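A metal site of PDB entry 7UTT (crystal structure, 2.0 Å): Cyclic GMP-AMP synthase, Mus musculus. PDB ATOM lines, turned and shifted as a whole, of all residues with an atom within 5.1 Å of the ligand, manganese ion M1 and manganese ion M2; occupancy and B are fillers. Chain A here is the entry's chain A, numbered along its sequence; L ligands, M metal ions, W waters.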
ATOM      1  N   THR A  54     -22.792  12.661 -15.915  1.00  0.00           N
ATOM      2  CA  THR A  54     -21.626  13.329 -15.331  1.00  0.00           C
ATOM      3  C   THR A  54     -21.606  13.149 -13.806  1.00  0.00           C
ATOM      4  O   THR A  54     -22.474  12.500 -13.219  1.00  0.00           O
ATOM      5  CB  THR A  54     -21.617  14.853 -15.661  1.00  0.00           C
ATOM      6  OG1 THR A  54     -22.800  15.434 -15.126  1.00  0.00           O
ATOM      7  CG2 THR A  54     -21.651  15.109 -17.099  1.00  0.00           C
ATOM      8  N   GLY A  55     -20.594  13.736 -13.149  1.00  0.00           N
ATOM      9  CA  GLY A  55     -20.543  13.738 -11.712  1.00  0.00           C
ATOM     10  C   GLY A  55     -19.971  12.458 -11.168  1.00  0.00           C
ATOM     11  O   GLY A  55     -19.524  11.584 -11.939  1.00  0.00           O
ATOM     12  N   SER A  56     -19.972  12.337  -9.823  1.00  0.00           N
ATOM     13  CA  SER A  56     -19.142  11.337  -9.160  1.00  0.00           C
ATOM     14  C   SER A  56     -19.457   9.895  -9.523  1.00  0.00           C
ATOM     15  O   SER A  56     -18.551   9.035  -9.534  1.00  0.00           O
ATOM     16  CB  SER A  56     -19.196  11.494  -7.648  1.00  0.00           C
ATOM     17  OG  SER A  56     -20.526  11.345  -7.156  1.00  0.00           O
ATOM     18  N   GLU A  59     -17.863   9.068 -12.799  1.00  0.00           N
ATOM     19  CA  GLU A  59     -16.410   9.147 -12.619  1.00  0.00           C
ATOM     20  C   GLU A  59     -15.842   8.052 -11.720  1.00  0.00           C
ATOM     21  O   GLU A  59     -14.647   8.006 -11.488  1.00  0.00           O
ATOM     22  CB  GLU A  59     -16.073  10.527 -12.009  1.00  0.00           C
ATOM     23  CG  GLU A  59     -16.451  11.689 -12.931  1.00  0.00           C
ATOM     24  CD  GLU A  59     -16.410  13.039 -12.247  1.00  0.00           C
ATOM     25  OE1 GLU A  59     -16.542  13.122 -11.003  1.00  0.00           O
ATOM     26  OE2 GLU A  59     -16.207  14.047 -12.972  1.00  0.00           O
ATOM     27  N   VAL A  61     -16.143   7.885  -8.485  1.00  0.00           N
ATOM     28  CA  VAL A  61     -15.720   8.397  -7.172  1.00  0.00           C
ATOM     29  C   VAL A  61     -16.921   8.694  -6.246  1.00  0.00           C
ATOM     30  O   VAL A  61     -16.764   9.366  -5.253  1.00  0.00           O
ATOM     31  CB  VAL A  61     -14.755   9.605  -7.290  1.00  0.00           C
ATOM     32  CG1 VAL A  61     -13.458   9.178  -7.966  1.00  0.00           C
ATOM     33  CG2 VAL A  61     -15.372  10.732  -8.080  1.00  0.00           C
ATOM     34  N   LYS A  62     -18.103   8.129  -6.546  1.00  0.00           N
ATOM     35  CA  LYS A  62     -19.223   8.187  -5.612  1.00  0.00           C
ATOM     36  C   LYS A  62     -18.884   7.292  -4.424  1.00  0.00           C
ATOM     37  O   LYS A  62     -18.395   6.177  -4.603  1.00  0.00           O
ATOM     38  CB  LYS A  62     -20.508   7.676  -6.254  1.00  0.00           C
ATOM     39  CG  LYS A  62     -21.734   7.808  -5.348  1.00  0.00           C
ATOM     40  CD  LYS A  62     -22.268   9.224  -5.349  1.00  0.00           C
ATOM     41  CE  LYS A  62     -23.454   9.405  -4.418  1.00  0.00           C
ATOM     42  NZ  LYS A  62     -23.186   9.025  -3.019  1.00  0.00           N
ATOM     43  N   GLU A  68     -26.949   9.318  -5.512  1.00  0.00           N
ATOM     44  CA  GLU A  68     -27.006  10.626  -6.158  1.00  0.00           C
ATOM     45  C   GLU A  68     -26.361  10.615  -7.542  1.00  0.00           C
ATOM     46  O   GLU A  68     -25.166  10.346  -7.684  1.00  0.00           O
ATOM     47  CB  GLU A  68     -26.394  11.712  -5.237  1.00  0.00           C
ATOM     48  CG  GLU A  68     -26.874  13.138  -5.499  1.00  0.00           C
ATOM     49  CD  GLU A  68     -26.068  13.884  -6.510  1.00  0.00           C
ATOM     50  OE1 GLU A  68     -25.040  13.326  -6.998  1.00  0.00           O
ATOM     51  OE2 GLU A  68     -26.421  15.055  -6.831  1.00  0.00           O
ATOM     52  N   PHE A  69     -27.180  10.887  -8.551  1.00  0.00           N
ATOM     53  CA  PHE A  69     -26.808  10.760  -9.945  1.00  0.00           C
ATOM     54  C   PHE A  69     -27.008  12.090 -10.629  1.00  0.00           C
ATOM     55  O   PHE A  69     -28.025  12.739 -10.376  1.00  0.00           O
ATOM     56  CB  PHE A  69     -27.701   9.710 -10.645  1.00  0.00           C
ATOM     57  CG  PHE A  69     -27.508   8.304 -10.173  1.00  0.00           C
ATOM     58  CD1 PHE A  69     -28.068   7.869  -8.985  1.00  0.00           C
ATOM     59  CD2 PHE A  69     -26.820   7.383 -10.959  1.00  0.00           C
ATOM     60  CE1 PHE A  69     -27.931   6.563  -8.570  1.00  0.00           C
ATOM     61  CE2 PHE A  69     -26.689   6.059 -10.556  1.00  0.00           C
ATOM     62  CZ  PHE A  69     -27.220   5.657  -9.332  1.00  0.00           C
ATOM     63  N   ASP A  70     -26.052  12.477 -11.481  1.00  0.00           N
ATOM     64  CA  ASP A  70     -26.107  13.705 -12.266  1.00  0.00           C
ATOM     65  C   ASP A  70     -26.161  13.441 -13.774  1.00  0.00           C
ATOM     66  O   ASP A  70     -25.368  12.662 -14.297  1.00  0.00           O
ATOM     67  CB  ASP A  70     -24.887  14.552 -11.941  1.00  0.00           C
ATOM     68  CG  ASP A  70     -24.752  14.771 -10.468  1.00  0.00           C
ATOM     69  OD1 ASP A  70     -25.647  15.461  -9.928  1.00  0.00           O
ATOM     70  OD2 ASP A  70     -23.778  14.224  -9.853  1.00  0.00           O
ATOM     71  N   ASP A 164     -30.239  14.617 -10.367  1.00  0.00           N
ATOM     72  CA  ASP A 164     -30.189  15.995 -10.819  1.00  0.00           C
ATOM     73  C   ASP A 164     -30.222  15.986 -12.352  1.00  0.00           C
ATOM     74  O   ASP A 164     -29.293  15.509 -12.978  1.00  0.00           O
ATOM     75  CB  ASP A 164     -28.894  16.670 -10.343  1.00  0.00           C
ATOM     76  CG  ASP A 164     -28.930  17.015  -8.848  1.00  0.00           C
ATOM     77  OD1 ASP A 164     -30.021  16.912  -8.213  1.00  0.00           O
ATOM     78  OD2 ASP A 164     -27.873  17.378  -8.301  1.00  0.00           O
ATOM     79  N   ARG A 221     -24.016  30.076 -16.330  1.00  0.00           N
ATOM     80  CA  ARG A 221     -22.670  29.754 -15.782  1.00  0.00           C
ATOM     81  C   ARG A 221     -22.022  28.647 -16.623  1.00  0.00           C
ATOM     82  O   ARG A 221     -22.738  27.708 -17.044  1.00  0.00           O
ATOM     83  CB  ARG A 221     -22.833  29.334 -14.314  1.00  0.00           C
ATOM     84  CG  ARG A 221     -21.521  29.129 -13.558  1.00  0.00           C
ATOM     85  CD  ARG A 221     -21.648  28.010 -12.550  1.00  0.00           C
ATOM     86  NE  ARG A 221     -21.260  26.775 -13.181  1.00  0.00           N
ATOM     87  CZ  ARG A 221     -21.728  25.573 -12.921  1.00  0.00           C
ATOM     88  NH1 ARG A 221     -22.683  25.375 -12.031  1.00  0.00           N
ATOM     89  NH2 ARG A 221     -21.249  24.548 -13.581  1.00  0.00           N
ATOM     90  N   LEU A 222     -20.709  28.749 -16.827  1.00  0.00           N
ATOM     91  CA  LEU A 222     -19.930  27.762 -17.582  1.00  0.00           C
ATOM     92  C   LEU A 222     -19.843  26.461 -16.856  1.00  0.00           C
ATOM     93  O   LEU A 222     -19.667  26.455 -15.644  1.00  0.00           O
ATOM     94  CB  LEU A 222     -18.493  28.274 -17.867  1.00  0.00           C
ATOM     95  CG  LEU A 222     -18.346  29.451 -18.821  1.00  0.00           C
ATOM     96  CD1 LEU A 222     -16.889  29.929 -18.970  1.00  0.00           C
ATOM     97  CD2 LEU A 222     -18.877  29.017 -20.174  1.00  0.00           C
ATOM     98  N   SER A 223     -20.013  25.338 -17.588  1.00  0.00           N
ATOM     99  CA  SER A 223     -19.820  23.985 -17.054  1.00  0.00           C
ATOM    100  C   SER A 223     -18.837  23.213 -17.921  1.00  0.00           C
ATOM    101  O   SER A 223     -18.953  23.215 -19.166  1.00  0.00           O
ATOM    102  CB  SER A 223     -21.112  23.204 -17.061  1.00  0.00           C
ATOM    103  OG  SER A 223     -20.885  21.880 -16.635  1.00  0.00           O
ATOM    104  N   SER A 225     -18.176  19.838 -16.964  1.00  0.00           N
ATOM    105  CA  SER A 225     -18.418  18.565 -16.312  1.00  0.00           C
ATOM    106  C   SER A 225     -18.010  17.397 -17.195  1.00  0.00           C
ATOM    107  O   SER A 225     -17.541  16.377 -16.693  1.00  0.00           O
ATOM    108  CB  SER A 225     -19.913  18.443 -15.913  1.00  0.00           C
ATOM    109  OG  SER A 225     -20.008  17.518 -14.907  1.00  0.00           O
ATOM    110  N   GLU A 228     -14.110  17.343 -16.978  1.00  0.00           N
ATOM    111  CA  GLU A 228     -13.803  16.797 -15.671  1.00  0.00           C
ATOM    112  C   GLU A 228     -13.946  15.281 -15.618  1.00  0.00           C
ATOM    113  O   GLU A 228     -13.099  14.600 -15.079  1.00  0.00           O
ATOM    114  CB  GLU A 228     -14.665  17.472 -14.614  1.00  0.00           C
ATOM    115  CG  GLU A 228     -14.353  18.952 -14.426  1.00  0.00           C
ATOM    116  CD  GLU A 228     -15.349  19.652 -13.506  1.00  0.00           C
ATOM    117  OE1 GLU A 228     -16.083  18.919 -12.795  1.00  0.00           O
ATOM    118  OE2 GLU A 228     -15.400  20.909 -13.537  1.00  0.00           O
ATOM    119  N   LYS A 259     -13.439  13.646   0.161  1.00  0.00           N
ATOM    120  CA  LYS A 259     -14.883  13.833   0.044  1.00  0.00           C
ATOM    121  C   LYS A 259     -15.595  13.343   1.290  1.00  0.00           C
ATOM    122  O   LYS A 259     -16.498  13.996   1.782  1.00  0.00           O
ATOM    123  CB  LYS A 259     -15.488  13.106  -1.152  1.00  0.00           C
ATOM    124  CG  LYS A 259     -15.086  13.623  -2.498  1.00  0.00           C
ATOM    125  CD  LYS A 259     -15.271  12.533  -3.578  1.00  0.00           C
ATOM    126  CE  LYS A 259     -16.718  11.973  -3.684  1.00  0.00           C
ATOM    127  NZ  LYS A 259     -17.624  13.016  -4.148  1.00  0.00           N
ATOM    128  N   GLU A 263     -18.044  15.331   3.803  1.00  0.00           N
ATOM    129  CA  GLU A 263     -19.425  14.810   3.940  1.00  0.00           C
ATOM    130  C   GLU A 263     -19.770  14.589   5.427  1.00  0.00           C
ATOM    131  O   GLU A 263     -20.823  15.001   5.901  1.00  0.00           O
ATOM    132  CB  GLU A 263     -19.706  13.497   3.148  1.00  0.00           C
ATOM    133  CG  GLU A 263     -19.843  13.621   1.600  1.00  0.00           C
ATOM    134  CD  GLU A 263     -20.410  12.347   0.866  1.00  0.00           C
ATOM    135  OE1 GLU A 263     -21.029  11.482   1.561  1.00  0.00           O
ATOM    136  OE2 GLU A 263     -20.236  12.186  -0.418  1.00  0.00           O
ATOM    137  N   SER A 277     -18.692  19.402  -2.293  1.00  0.00           N
ATOM    138  CA  SER A 277     -17.684  18.462  -2.753  1.00  0.00           C
ATOM    139  C   SER A 277     -16.851  19.022  -3.927  1.00  0.00           C
ATOM    140  O   SER A 277     -15.670  18.668  -4.101  1.00  0.00           O
ATOM    141  CB  SER A 277     -18.303  17.106  -3.106  1.00  0.00           C
ATOM    142  OG  SER A 277     -19.186  17.250  -4.192  1.00  0.00           O
ATOM    143  N   TYR A 278     -17.434  19.947  -4.706  1.00  0.00           N
ATOM    144  CA  TYR A 278     -16.729  20.574  -5.860  1.00  0.00           C
ATOM    145  C   TYR A 278     -15.507  21.377  -5.376  1.00  0.00           C
ATOM    146  O   TYR A 278     -14.551  21.528  -6.125  1.00  0.00           O
ATOM    147  CB  TYR A 278     -17.670  21.443  -6.692  1.00  0.00           C
ATOM    148  CG  TYR A 278     -17.054  21.824  -8.018  1.00  0.00           C
ATOM    149  CD1 TYR A 278     -16.865  20.871  -9.000  1.00  0.00           C
ATOM    150  CD2 TYR A 278     -16.642  23.127  -8.281  1.00  0.00           C
ATOM    151  CE1 TYR A 278     -16.297  21.212 -10.219  1.00  0.00           C
ATOM    152  CE2 TYR A 278     -16.031  23.478  -9.489  1.00  0.00           C
ATOM    153  CZ  TYR A 278     -15.874  22.500 -10.466  1.00  0.00           C
ATOM    154  OH  TYR A 278     -15.336  22.796 -11.688  1.00  0.00           O
ATOM    155  N   LYS A 281     -12.939  18.635  -5.153  1.00  0.00           N
ATOM    156  CA  LYS A 281     -12.606  18.221  -6.522  1.00  0.00           C
ATOM    157  C   LYS A 281     -11.653  19.216  -7.167  1.00  0.00           C
ATOM    158  O   LYS A 281     -10.642  18.854  -7.829  1.00  0.00           O
ATOM    159  CB  LYS A 281     -13.872  18.039  -7.375  1.00  0.00           C
ATOM    160  CG  LYS A 281     -13.654  17.294  -8.677  1.00  0.00           C
ATOM    161  CD  LYS A 281     -14.928  17.296  -9.513  1.00  0.00           C
ATOM    162  CE  LYS A 281     -14.890  16.174 -10.564  1.00  0.00           C
ATOM    163  NZ  LYS A 281     -16.012  16.244 -11.560  1.00  0.00           N
ATOM    164  N   HIS A 324     -10.898  28.421  -9.545  1.00  0.00           N
ATOM    165  CA  HIS A 324     -11.585  27.506 -10.428  1.00  0.00           C
ATOM    166  C   HIS A 324     -10.558  26.957 -11.410  1.00  0.00           C
ATOM    167  O   HIS A 324      -9.723  27.712 -11.911  1.00  0.00           O
ATOM    168  CB  HIS A 324     -12.669  28.297 -11.164  1.00  0.00           C
ATOM    169  CG  HIS A 324     -13.686  27.459 -11.835  1.00  0.00           C
ATOM    170  ND1 HIS A 324     -13.411  26.742 -12.986  1.00  0.00           N
ATOM    171  CD2 HIS A 324     -14.977  27.221 -11.536  1.00  0.00           C
ATOM    172  CE1 HIS A 324     -14.493  26.078 -13.341  1.00  0.00           C
ATOM    173  NE2 HIS A 324     -15.463  26.354 -12.481  1.00  0.00           N
HETATM  174  P1  LIG L   1     -20.955  14.032  -5.140  1.00  0.00           P
HETATM  175  O1  LIG L   1     -20.505  12.644  -4.777  1.00  0.00           O
HETATM  176  O2  LIG L   1     -20.694  14.973  -4.007  1.00  0.00           O
HETATM  177  O3  LIG L   1     -22.356  14.075  -5.725  1.00  0.00           O
HETATM  178  P2  LIG L   1     -20.193  15.462  -7.447  1.00  0.00           P
HETATM  179  O4  LIG L   1     -21.044  14.693  -8.400  1.00  0.00           O
HETATM  180  O5  LIG L   1     -18.950  15.837  -8.251  1.00  0.00           O
HETATM  181  O6  LIG L   1     -19.857  14.495  -6.237  1.00  0.00           O
HETATM  182  P3  LIG L   1     -22.563  17.507  -7.720  1.00  0.00           P
HETATM  183  O7  LIG L   1     -23.586  16.412  -7.857  1.00  0.00           O
HETATM  184  O8  LIG L   1     -23.031  18.647  -6.897  1.00  0.00           O
HETATM  185  C1  LIG L   1     -21.230  16.698  -7.210  1.00  0.00           C
HETATM  186  O9  LIG L   1     -22.162  18.027  -9.201  1.00  0.00           O
HETATM  187  C2  LIG L   1     -22.119  17.239 -10.391  1.00  0.00           C
HETATM  188  C3  LIG L   1     -21.075  17.782 -11.364  1.00  0.00           C
HETATM  189  O10 LIG L   1     -21.478  19.072 -11.863  1.00  0.00           O
HETATM  190  C4  LIG L   1     -19.688  17.968 -10.709  1.00  0.00           C
HETATM  191  O11 LIG L   1     -18.940  16.730 -10.706  1.00  0.00           O
HETATM  192  C5  LIG L   1     -19.128  19.064 -11.597  1.00  0.00           C
HETATM  193  O12 LIG L   1     -18.616  18.508 -12.815  1.00  0.00           O
HETATM  194  C6  LIG L   1     -20.334  19.938 -11.925  1.00  0.00           C
HETATM  195  N1  LIG L   1     -20.488  21.057 -10.955  1.00  0.00           N
HETATM  196  C7  LIG L   1     -21.234  21.061  -9.828  1.00  0.00           C
HETATM  197  N2  LIG L   1     -21.122  22.258  -9.205  1.00  0.00           N
HETATM  198  C8  LIG L   1     -20.282  23.009  -9.972  1.00  0.00           C
HETATM  199  C9  LIG L   1     -19.800  24.320  -9.867  1.00  0.00           C
HETATM  200  N3  LIG L   1     -20.148  25.119  -8.820  1.00  0.00           N
HETATM  201  N4  LIG L   1     -18.956  24.780 -10.805  1.00  0.00           N
HETATM  202  C10 LIG L   1     -18.576  24.016 -11.853  1.00  0.00           C
HETATM  203  N5  LIG L   1     -19.040  22.759 -11.988  1.00  0.00           N
HETATM  204  C11 LIG L   1     -19.894  22.250 -11.064  1.00  0.00           C
HETATM  205 MN    MN M   1     -25.746  16.580  -8.108  1.00  0.00          MN
HETATM  206 MN    MN M   2     -23.189  14.137  -7.770  1.00  0.00          MN
HETATM  207  O   HOH W   1     -17.475  17.193  -6.587  1.00  0.00           O
HETATM  208  O   HOH W   2     -22.897  11.835  -8.126  1.00  0.00           O
HETATM  209  O   HOH W   3     -16.808  14.087  -8.560  1.00  0.00           O
HETATM  210  O   HOH W   4     -22.168  21.987 -13.839  1.00  0.00           O
HETATM  211  O   HOH W   5     -25.544  17.857  -6.360  1.00  0.00           O
HETATM  212  O   HOH W   6     -17.585  22.328 -14.473  1.00  0.00           O
HETATM  213  O   HOH W   7     -25.431  18.392  -9.137  1.00  0.00           O
HETATM  214  O   HOH W   8     -20.514  10.759  -2.986  1.00  0.00           O
HETATM  215  O   HOH W   9     -24.367  15.799  -4.624  1.00  0.00           O
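Ser 56 touches manganese ion M2.
Within 4 Å of manganese ion M2: Ser 56, Glu 68 and Asp 70.
The nearest printed residue that does not touch manganese ion M2 is Gly 55 (4.8 Å).
The nearest printed residue that does not touch manganese ion M1 is Phe 69 (5.0 Å).
Water W2 bridges OG of Ser 56 and O of Glu 68.
Water W8 lies within hydrogen-bond range of O1 of the ligand (2.6 Å), OE2 of Glu 263 (3.0 Å) and NZ of Lys 62 (3.2 Å).
Water W1 lies within hydrogen-bond range of an oxygen (O5) of the ligand (2.6 Å), the side-chain hydroxyl (OG) of Ser 277 (2.9 Å) and the backbone NH (N) of Tyr 278 (3.3 Å).
Water W3 bridges OE1 of Glu 59 and O5 of the ligand.
Water W6 lies within hydrogen-bond range of the side-chain carboxylate of Glu 228 (2.8 Å) and a nitrogen (N5) of the ligand (2.9 Å).
Water W4 bridges NH2 of Arg 221 (2.7 Å) and OG of Ser 223 (3.1 Å).
The backbone carbonyl oxygen (O) of Ser 56 lies within hydrogen-bond range of the backbone NH (N) of Lys 62 (3.2 Å).
N of Val 61 is in hydrogen-bond range of O of Ser 56 (2.9 Å).
The backbone NH (N) of Asp 164 sits at hydrogen-bond distance from the backbone carbonyl oxygen (O) of Phe 69 (2.9 Å).
The side-chain carboxylate of Glu 228 lies within hydrogen-bond range of the side-chain hydroxyl of Tyr 278 (2.6 Å).
The side-chain hydroxyl of Ser 225 lies close to the side-chain hydroxyl of Thr 54, at 3.5 Å.
The side-chain carboxylate of Glu 59 lies within salt-bridge range of the side-chain amino group of Lys 281, 2.6 Å away.
The backbone NH (N) of Ser 225 is in hydrogen-bond range of the side-chain hydroxyl (OG) of Ser 223 (3.4 Å).
The side-chain carboxylate of Glu 228 is in salt-bridge range of the side-chain amino group of Lys 281, at 2.9 Å.
Manganese ion M2 is bound by OE1 of Glu 68, OD2 of Asp 70, O3 of the ligand, O4 of the ligand, O7 of the ligand and water W2.
Manganese ion M2 has six donor atoms within binding distance.
The side-chain amino group of Lys 259 is in salt-bridge range of an oxygen (O1) of the ligand, 3.0 Å away.
OG of Ser 225 is in hydrogen-bond range of O12 of the ligand.
O4 of the ligand lies close to N of Ser 56 (3.0 Å).
The side-chain amino group of Lys 281 lies within hydrogen-bond range of an oxygen (O11) of the ligand.
O2 of the ligand is in hydrogen-bond range of OG of Ser 277 (2.7 Å).
OE1 of Glu 228 sits at hydrogen-bond distance from O12 of the ligand, at 2.6 Å.
An oxygen (O1) of the ligand is in hydrogen-bond range of the side-chain hydroxyl (OG) of Ser 56.
N5 of the ligand sits close to NH2 of Arg 221 (3.3 Å).
OE2 of Glu 68 is bound to manganese ion M1 (2.1 Å).
Water W7 binds manganese ion M1, 2.1 Å away.
Manganese ion M1 is bound by OD1 of Asp 70.
Water W5 binds manganese ion M1.
O7 of the ligand binds manganese ion M1 (2.2 Å).
Manganese ion M1 is bound by OD2 of Asp 164 (2.3 Å).
Merely in contact with the ligand: Gly 55, Lys 62, Tyr 278 and His 324.
Hydrophobic or aromatic side chains within 4 Å of the ligand: Tyr 278.
Of the 21 residues printed, 13 come within 4 Å of the ligand.
The nearest printed residue that does not touch the ligand is Glu 59 (4.3 Å).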
